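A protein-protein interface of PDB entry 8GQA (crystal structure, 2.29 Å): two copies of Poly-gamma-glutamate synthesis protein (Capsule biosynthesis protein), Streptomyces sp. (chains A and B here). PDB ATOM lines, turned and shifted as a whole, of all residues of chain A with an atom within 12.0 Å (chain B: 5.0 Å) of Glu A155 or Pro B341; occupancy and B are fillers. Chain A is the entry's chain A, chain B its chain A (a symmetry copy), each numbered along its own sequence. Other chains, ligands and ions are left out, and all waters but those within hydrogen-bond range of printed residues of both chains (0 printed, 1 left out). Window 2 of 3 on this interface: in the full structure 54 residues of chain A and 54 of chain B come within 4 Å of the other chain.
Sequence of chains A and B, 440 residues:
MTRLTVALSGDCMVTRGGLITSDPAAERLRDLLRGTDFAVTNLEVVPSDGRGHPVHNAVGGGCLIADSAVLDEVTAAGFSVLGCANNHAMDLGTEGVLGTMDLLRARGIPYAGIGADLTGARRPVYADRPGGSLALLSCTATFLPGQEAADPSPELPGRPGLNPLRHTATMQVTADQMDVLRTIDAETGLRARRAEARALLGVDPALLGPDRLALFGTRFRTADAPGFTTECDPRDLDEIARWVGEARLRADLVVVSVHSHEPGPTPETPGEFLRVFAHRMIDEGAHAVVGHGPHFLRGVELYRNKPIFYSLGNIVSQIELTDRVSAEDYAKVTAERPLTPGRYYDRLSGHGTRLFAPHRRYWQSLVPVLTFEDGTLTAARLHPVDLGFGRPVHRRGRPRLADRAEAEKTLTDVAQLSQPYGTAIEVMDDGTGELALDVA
No position is printed for both chains.
Of the 8 pairs that touch across the chains among the printed residues, none has its exchanged pair printed and touching as well.
Of the 10 printed residues of chain A, 3 touch a printed residue of chain B.
Hydrophobic or aromatic side chains of chain A that line the printed part of chain B: Leu A156.
Of the 12 printed residues of chain B, 5 touch a printed residue of chain A.
Printed residues of chain B that touch a printed residue of chain A: Asp B323, Arg B324, Val B325, Tyr B330 and Pro B341.
Hydrophobic or aromatic side chains of chain B within 4 Å of the printed part of chain A: Tyr B330 and Pro B341.
Among the printed residues, no Asp or Glu carboxylate lies within 4 Å of a Lys or Arg side-chain nitrogen of the other chain.
Asp A151 touches none of the printed residues of chain B.
Printed residues of chain B within 4 Å of Ser A153: Val B325 (2.7 Å).
Glu A155 touches just these residues of chain B: Asp B323 (3.1 Å), Arg B324 (3.97 Å), Val B325 (3.6 Å), Tyr B330 (2.9 Å) and Pro B341 (3.8 Å).
Printed residues of chain B within 4 Å of Leu A156: Arg B324 (3.7 Å) and Val B325 (3.7 Å).
Thr B322 touches none of the printed residues of chain A.
Asp B323 touches just one residue of chain A: Glu A155.
Arg B324 touches just these residues of chain A: Glu A155 (3.97 Å) and Leu A156 (3.7 Å).
No residue of chain A comes within 4 Å of Leu B339.
Of chain A, only Glu A155 (3.8 Å) comes within 4 Å of Pro B341.
No residue of chain A comes within 4 Å of Gly B342.
Tyr B345 touches none of the printed residues of chain A.
The nearest printed residue of chain B that does not touch Glu A155 is Leu B339 (5.2 Å).
The nearest printed residue of chain B that does not touch Leu A156 is Asp B323 (6.3 Å).
The side-chain hydroxyl (OG) of Ser A153 is in hydrogen-bond range of the backbone NH (N) of Leu A156 (3.0 Å).
The side-chain hydroxyl of Ser A153 lies close to the backbone NH of Glu A155.
O of Leu B339 sits close to OH of Tyr B330 (3.4 Å).
OE1 of Glu A155 lies within hydrogen-bond range of OH of Tyr B330 (2.9 Å).
The side-chain hydroxyl (OG) of Ser A153 sits at hydrogen-bond distance from the backbone carbonyl oxygen (O) of Val B325 (2.7 Å).
Glu A155 touches Asp B323.
CA of Arg B324 touches CB of Glu A155, 3.97 Å away.
Val B325 touches Glu A155 (O to OE1, 3.6 Å).
OE2 of Glu A155 touches CD of Pro B341 (3.8 Å).
Leu A156 touches Arg B324.
Val B325 touches Leu A156 (C to CD1, 3.7 Å).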
ATOM      1  N   ALA A 150     -15.733 -16.111 -30.408  1.00  0.00           N
ATOM      2  CA  ALA A 150     -15.894 -14.956 -29.540  1.00  0.00           C
ATOM      3  C   ALA A 150     -14.884 -15.032 -28.407  1.00  0.00           C
ATOM      4  O   ALA A 150     -14.550 -16.117 -27.923  1.00  0.00           O
ATOM      5  CB  ALA A 150     -17.318 -14.866 -28.972  1.00  0.00           C
ATOM      6  N   ASP A 151     -14.392 -13.873 -28.000  1.00  0.00           N
ATOM      7  CA  ASP A 151     -13.467 -13.777 -26.885  1.00  0.00           C
ATOM      8  C   ASP A 151     -14.231 -13.710 -25.570  1.00  0.00           C
ATOM      9  O   ASP A 151     -15.420 -13.374 -25.547  1.00  0.00           O
ATOM     10  CB  ASP A 151     -12.579 -12.546 -27.052  1.00  0.00           C
ATOM     11  CG  ASP A 151     -11.259 -12.873 -27.723  1.00  0.00           C
ATOM     12  OD1 ASP A 151     -10.872 -14.062 -27.722  1.00  0.00           O
ATOM     13  OD2 ASP A 151     -10.610 -11.945 -28.249  1.00  0.00           O
ATOM     14  N   PRO A 152     -13.591 -14.040 -24.453  1.00  0.00           N
ATOM     15  CA  PRO A 152     -14.298 -14.019 -23.170  1.00  0.00           C
ATOM     16  C   PRO A 152     -14.496 -12.603 -22.649  1.00  0.00           C
ATOM     17  O   PRO A 152     -13.796 -11.659 -23.021  1.00  0.00           O
ATOM     18  CB  PRO A 152     -13.381 -14.820 -22.232  1.00  0.00           C
ATOM     19  CG  PRO A 152     -12.299 -15.402 -23.104  1.00  0.00           C
ATOM     20  CD  PRO A 152     -12.209 -14.527 -24.304  1.00  0.00           C
ATOM     21  N   SER A 153     -15.483 -12.478 -21.779  1.00  0.00           N
ATOM     22  CA  SER A 153     -15.747 -11.295 -20.983  1.00  0.00           C
ATOM     23  C   SER A 153     -15.382 -11.582 -19.531  1.00  0.00           C
ATOM     24  O   SER A 153     -15.059 -12.719 -19.175  1.00  0.00           O
ATOM     25  CB  SER A 153     -17.225 -10.899 -21.104  1.00  0.00           C
ATOM     26  OG  SER A 153     -18.025 -11.610 -20.177  1.00  0.00           O
ATOM     27  N   PRO A 154     -15.392 -10.565 -18.661  1.00  0.00           N
ATOM     28  CA  PRO A 154     -15.123 -10.832 -17.237  1.00  0.00           C
ATOM     29  C   PRO A 154     -16.070 -11.837 -16.600  1.00  0.00           C
ATOM     30  O   PRO A 154     -15.704 -12.443 -15.585  1.00  0.00           O
ATOM     31  CB  PRO A 154     -15.265  -9.448 -16.593  1.00  0.00           C
ATOM     32  CG  PRO A 154     -14.864  -8.511 -17.670  1.00  0.00           C
ATOM     33  CD  PRO A 154     -15.386  -9.117 -18.948  1.00  0.00           C
ATOM     34  N   GLU A 155     -17.264 -12.048 -17.158  1.00  0.00           N
ATOM     35  CA  GLU A 155     -18.259 -12.912 -16.540  1.00  0.00           C
ATOM     36  C   GLU A 155     -18.606 -14.158 -17.338  1.00  0.00           C
ATOM     37  O   GLU A 155     -19.138 -15.108 -16.754  1.00  0.00           O
ATOM     38  CB  GLU A 155     -19.559 -12.133 -16.281  1.00  0.00           C
ATOM     39  CG  GLU A 155     -19.409 -11.027 -15.266  1.00  0.00           C
ATOM     40  CD  GLU A 155     -19.075  -9.695 -15.900  1.00  0.00           C
ATOM     41  OE1 GLU A 155     -19.392  -9.509 -17.095  1.00  0.00           O
ATOM     42  OE2 GLU A 155     -18.497  -8.834 -15.204  1.00  0.00           O
ATOM     43  N   LEU A 156     -18.337 -14.187 -18.637  1.00  0.00           N
ATOM     44  CA  LEU A 156     -18.707 -15.328 -19.454  1.00  0.00           C
ATOM     45  C   LEU A 156     -17.519 -15.784 -20.284  1.00  0.00           C
ATOM     46  O   LEU A 156     -16.662 -14.973 -20.650  1.00  0.00           O
ATOM     47  CB  LEU A 156     -19.880 -14.986 -20.385  1.00  0.00           C
ATOM     48  CG  LEU A 156     -21.234 -14.766 -19.705  1.00  0.00           C
ATOM     49  CD1 LEU A 156     -22.256 -14.236 -20.698  1.00  0.00           C
ATOM     50  CD2 LEU A 156     -21.725 -16.052 -19.059  1.00  0.00           C
ATOM     51  N   PRO A 157     -17.437 -17.075 -20.590  1.00  0.00           N
ATOM     52  CA  PRO A 157     -16.375 -17.555 -21.477  1.00  0.00           C
ATOM     53  C   PRO A 157     -16.584 -17.051 -22.895  1.00  0.00           C
ATOM     54  O   PRO A 157     -17.597 -16.438 -23.236  1.00  0.00           O
ATOM     55  CB  PRO A 157     -16.510 -19.078 -21.405  1.00  0.00           C
ATOM     56  CG  PRO A 157     -17.942 -19.304 -21.051  1.00  0.00           C
ATOM     57  CD  PRO A 157     -18.310 -18.172 -20.132  1.00  0.00           C
ATOM     58  N   GLY A 158     -15.594 -17.325 -23.731  1.00  0.00           N
ATOM     59  CA  GLY A 158     -15.709 -17.068 -25.149  1.00  0.00           C
ATOM     60  C   GLY A 158     -16.601 -18.096 -25.813  1.00  0.00           C
ATOM     61  O   GLY A 158     -17.350 -18.830 -25.164  1.00  0.00           O
ATOM     62  N   ARG A 159     -16.516 -18.143 -27.140  1.00  0.00           N
ATOM     63  CA  ARG A 159     -17.241 -19.129 -27.917  1.00  0.00           C
ATOM     64  C   ARG A 159     -16.286 -19.722 -28.947  1.00  0.00           C
ATOM     65  O   ARG A 159     -15.636 -18.971 -29.694  1.00  0.00           O
ATOM     66  CB  ARG A 159     -18.467 -18.517 -28.610  1.00  0.00           C
ATOM     67  CG  ARG A 159     -19.213 -19.500 -29.500  1.00  0.00           C
ATOM     68  CD  ARG A 159     -20.425 -18.860 -30.156  1.00  0.00           C
ATOM     69  NE  ARG A 159     -20.051 -17.809 -31.096  1.00  0.00           N
ATOM     70  CZ  ARG A 159     -20.244 -16.512 -30.881  1.00  0.00           C
ATOM     71  NH1 ARG A 159     -20.810 -16.100 -29.755  1.00  0.00           N
ATOM     72  NH2 ARG A 159     -19.871 -15.625 -31.794  1.00  0.00           N
ATOM     73  N   THR B 322     -28.905  -8.687 -14.737  1.00  0.00           N
ATOM     74  CA  THR B 322     -28.119  -9.886 -14.991  1.00  0.00           C
ATOM     75  C   THR B 322     -26.647  -9.635 -14.683  1.00  0.00           C
ATOM     76  O   THR B 322     -26.121  -8.540 -14.905  1.00  0.00           O
ATOM     77  CB  THR B 322     -28.291 -10.354 -16.439  1.00  0.00           C
ATOM     78  OG1 THR B 322     -27.675 -11.637 -16.605  1.00  0.00           O
ATOM     79  CG2 THR B 322     -27.657  -9.378 -17.407  1.00  0.00           C
ATOM     80  N   ASP B 323     -25.990 -10.655 -14.140  1.00  0.00           N
ATOM     81  CA  ASP B 323     -24.586 -10.581 -13.774  1.00  0.00           C
ATOM     82  C   ASP B 323     -23.669 -11.186 -14.826  1.00  0.00           C
ATOM     83  O   ASP B 323     -22.452 -11.212 -14.625  1.00  0.00           O
ATOM     84  CB  ASP B 323     -24.354 -11.283 -12.431  1.00  0.00           C
ATOM     85  CG  ASP B 323     -24.066 -10.312 -11.303  1.00  0.00           C
ATOM     86  OD1 ASP B 323     -23.892  -9.106 -11.582  1.00  0.00           O
ATOM     87  OD2 ASP B 323     -24.010 -10.756 -10.138  1.00  0.00           O
ATOM     88  N   ARG B 324     -24.218 -11.667 -15.942  1.00  0.00           N
ATOM     89  CA  ARG B 324     -23.458 -12.394 -16.959  1.00  0.00           C
ATOM     90  C   ARG B 324     -23.667 -11.705 -18.306  1.00  0.00           C
ATOM     91  O   ARG B 324     -24.623 -12.009 -19.027  1.00  0.00           O
ATOM     92  CB  ARG B 324     -23.887 -13.858 -17.004  1.00  0.00           C
ATOM     93  CG  ARG B 324     -23.608 -14.636 -15.725  1.00  0.00           C
ATOM     94  CD  ARG B 324     -24.644 -15.731 -15.521  1.00  0.00           C
ATOM     95  NE  ARG B 324     -24.152 -16.819 -14.677  1.00  0.00           N
ATOM     96  CZ  ARG B 324     -24.278 -16.858 -13.355  1.00  0.00           C
ATOM     97  NH1 ARG B 324     -24.881 -15.866 -12.712  1.00  0.00           N
ATOM     98  NH2 ARG B 324     -23.800 -17.890 -12.672  1.00  0.00           N
ATOM     99  N   VAL B 325     -22.770 -10.784 -18.647  1.00  0.00           N
ATOM    100  CA  VAL B 325     -22.811 -10.059 -19.912  1.00  0.00           C
ATOM    101  C   VAL B 325     -21.655 -10.545 -20.778  1.00  0.00           C
ATOM    102  O   VAL B 325     -20.503 -10.569 -20.329  1.00  0.00           O
ATOM    103  CB  VAL B 325     -22.739  -8.537 -19.695  1.00  0.00           C
ATOM    104  CG1 VAL B 325     -22.615  -7.813 -21.027  1.00  0.00           C
ATOM    105  CG2 VAL B 325     -23.964  -8.054 -18.932  1.00  0.00           C
ATOM    106  N   TYR B 330     -20.954  -6.480 -24.527  1.00  0.00           N
ATOM    107  CA  TYR B 330     -20.207  -5.321 -24.043  1.00  0.00           C
ATOM    108  C   TYR B 330     -19.774  -4.419 -25.193  1.00  0.00           C
ATOM    109  O   TYR B 330     -19.730  -3.192 -25.047  1.00  0.00           O
ATOM    110  CB  TYR B 330     -18.983  -5.778 -23.248  1.00  0.00           C
ATOM    111  CG  TYR B 330     -19.231  -6.032 -21.777  1.00  0.00           C
ATOM    112  CD1 TYR B 330     -19.663  -5.013 -20.937  1.00  0.00           C
ATOM    113  CD2 TYR B 330     -19.011  -7.288 -21.223  1.00  0.00           C
ATOM    114  CE1 TYR B 330     -19.883  -5.241 -19.590  1.00  0.00           C
ATOM    115  CE2 TYR B 330     -19.228  -7.525 -19.878  1.00  0.00           C
ATOM    116  CZ  TYR B 330     -19.664  -6.497 -19.066  1.00  0.00           C
ATOM    117  OH  TYR B 330     -19.881  -6.727 -17.726  1.00  0.00           O
ATOM    118  N   LEU B 339     -16.293  -2.034 -18.455  1.00  0.00           N
ATOM    119  CA  LEU B 339     -17.578  -1.784 -17.823  1.00  0.00           C
ATOM    120  C   LEU B 339     -17.977  -2.934 -16.908  1.00  0.00           C
ATOM    121  O   LEU B 339     -17.710  -4.103 -17.204  1.00  0.00           O
ATOM    122  CB  LEU B 339     -18.669  -1.574 -18.875  1.00  0.00           C
ATOM    123  CG  LEU B 339     -18.598  -0.294 -19.704  1.00  0.00           C
ATOM    124  CD1 LEU B 339     -19.805  -0.195 -20.620  1.00  0.00           C
ATOM    125  CD2 LEU B 339     -18.506   0.922 -18.798  1.00  0.00           C
ATOM    126  N   THR B 340     -18.610  -2.591 -15.799  1.00  0.00           N
ATOM    127  CA  THR B 340     -19.340  -3.537 -14.976  1.00  0.00           C
ATOM    128  C   THR B 340     -20.750  -3.702 -15.528  1.00  0.00           C
ATOM    129  O   THR B 340     -21.253  -2.822 -16.234  1.00  0.00           O
ATOM    130  CB  THR B 340     -19.382  -3.050 -13.529  1.00  0.00           C
ATOM    131  OG1 THR B 340     -19.991  -1.753 -13.474  1.00  0.00           O
ATOM    132  CG2 THR B 340     -17.975  -2.969 -12.955  1.00  0.00           C
ATOM    133  N   PRO B 341     -21.412  -4.831 -15.245  1.00  0.00           N
ATOM    134  CA  PRO B 341     -22.732  -5.076 -15.860  1.00  0.00           C
ATOM    135  C   PRO B 341     -23.743  -3.954 -15.667  1.00  0.00           C
ATOM    136  O   PRO B 341     -24.371  -3.520 -16.642  1.00  0.00           O
ATOM    137  CB  PRO B 341     -23.181  -6.375 -15.179  1.00  0.00           C
ATOM    138  CG  PRO B 341     -21.909  -7.082 -14.876  1.00  0.00           C
ATOM    139  CD  PRO B 341     -20.934  -6.003 -14.489  1.00  0.00           C
ATOM    140  N   GLY B 342     -23.915  -3.468 -14.435  1.00  0.00           N
ATOM    141  CA  GLY B 342     -24.889  -2.413 -14.196  1.00  0.00           C
ATOM    142  C   GLY B 342     -24.583  -1.141 -14.963  1.00  0.00           C
ATOM    143  O   GLY B 342     -25.487  -0.497 -15.501  1.00  0.00           O
ATOM    144  N   ARG B 343     -23.304  -0.762 -15.023  1.00  0.00           N
ATOM    145  CA  ARG B 343     -22.917   0.410 -15.804  1.00  0.00           C
ATOM    146  C   ARG B 343     -23.169   0.187 -17.289  1.00  0.00           C
ATOM    147  O   ARG B 343     -23.559   1.115 -18.008  1.00  0.00           O
ATOM    148  CB  ARG B 343     -21.447   0.745 -15.559  1.00  0.00           C
ATOM    149  CG  ARG B 343     -21.160   1.382 -14.211  1.00  0.00           C
ATOM    150  CD  ARG B 343     -19.689   1.746 -14.097  1.00  0.00           C
ATOM    151  NE  ARG B 343     -19.376   2.404 -12.833  1.00  0.00           N
ATOM    152  CZ  ARG B 343     -18.988   1.765 -11.735  1.00  0.00           C
ATOM    153  NH1 ARG B 343     -18.865   0.444 -11.743  1.00  0.00           N
ATOM    154  NH2 ARG B 343     -18.722   2.445 -10.628  1.00  0.00           N
ATOM    155  N   TYR B 344     -22.945  -1.040 -17.767  1.00  0.00           N
ATOM    156  CA  TYR B 344     -23.190  -1.347 -19.172  1.00  0.00           C
ATOM    157  C   TYR B 344     -24.657  -1.153 -19.532  1.00  0.00           C
ATOM    158  O   TYR B 344     -24.977  -0.582 -20.582  1.00  0.00           O
ATOM    159  CB  TYR B 344     -22.741  -2.778 -19.474  1.00  0.00           C
ATOM    160  CG  TYR B 344     -23.464  -3.439 -20.627  1.00  0.00           C
ATOM    161  CD1 TYR B 344     -23.077  -3.206 -21.939  1.00  0.00           C
ATOM    162  CD2 TYR B 344     -24.524  -4.310 -20.400  1.00  0.00           C
ATOM    163  CE1 TYR B 344     -23.730  -3.812 -22.997  1.00  0.00           C
ATOM    164  CE2 TYR B 344     -25.185  -4.919 -21.451  1.00  0.00           C
ATOM    165  CZ  TYR B 344     -24.783  -4.667 -22.747  1.00  0.00           C
ATOM    166  OH  TYR B 344     -25.437  -5.274 -23.795  1.00  0.00           O
ATOM    167  N   TYR B 345     -25.564  -1.610 -18.667  1.00  0.00           N
ATOM    168  CA  TYR B 345     -26.989  -1.476 -18.955  1.00  0.00           C
ATOM    169  C   TYR B 345     -27.442  -0.027 -18.846  1.00  0.00           C
ATOM    170  O   TYR B 345     -28.328   0.408 -19.591  1.00  0.00           O
ATOM    171  CB  TYR B 345     -27.797  -2.371 -18.019  1.00  0.00           C
ATOM    172  CG  TYR B 345     -27.881  -3.788 -18.521  1.00  0.00           C
ATOM    173  CD1 TYR B 345     -28.671  -4.103 -19.616  1.00  0.00           C
ATOM    174  CD2 TYR B 345     -27.151  -4.805 -17.922  1.00  0.00           C
ATOM    175  CE1 TYR B 345     -28.747  -5.393 -20.093  1.00  0.00           C
ATOM    176  CE2 TYR B 345     -27.219  -6.100 -18.392  1.00  0.00           C
ATOM    177  CZ  TYR B 345     -28.020  -6.387 -19.479  1.00  0.00           C
ATOM    178  OH  TYR B 345     -28.103  -7.670 -19.963  1.00  0.00           O
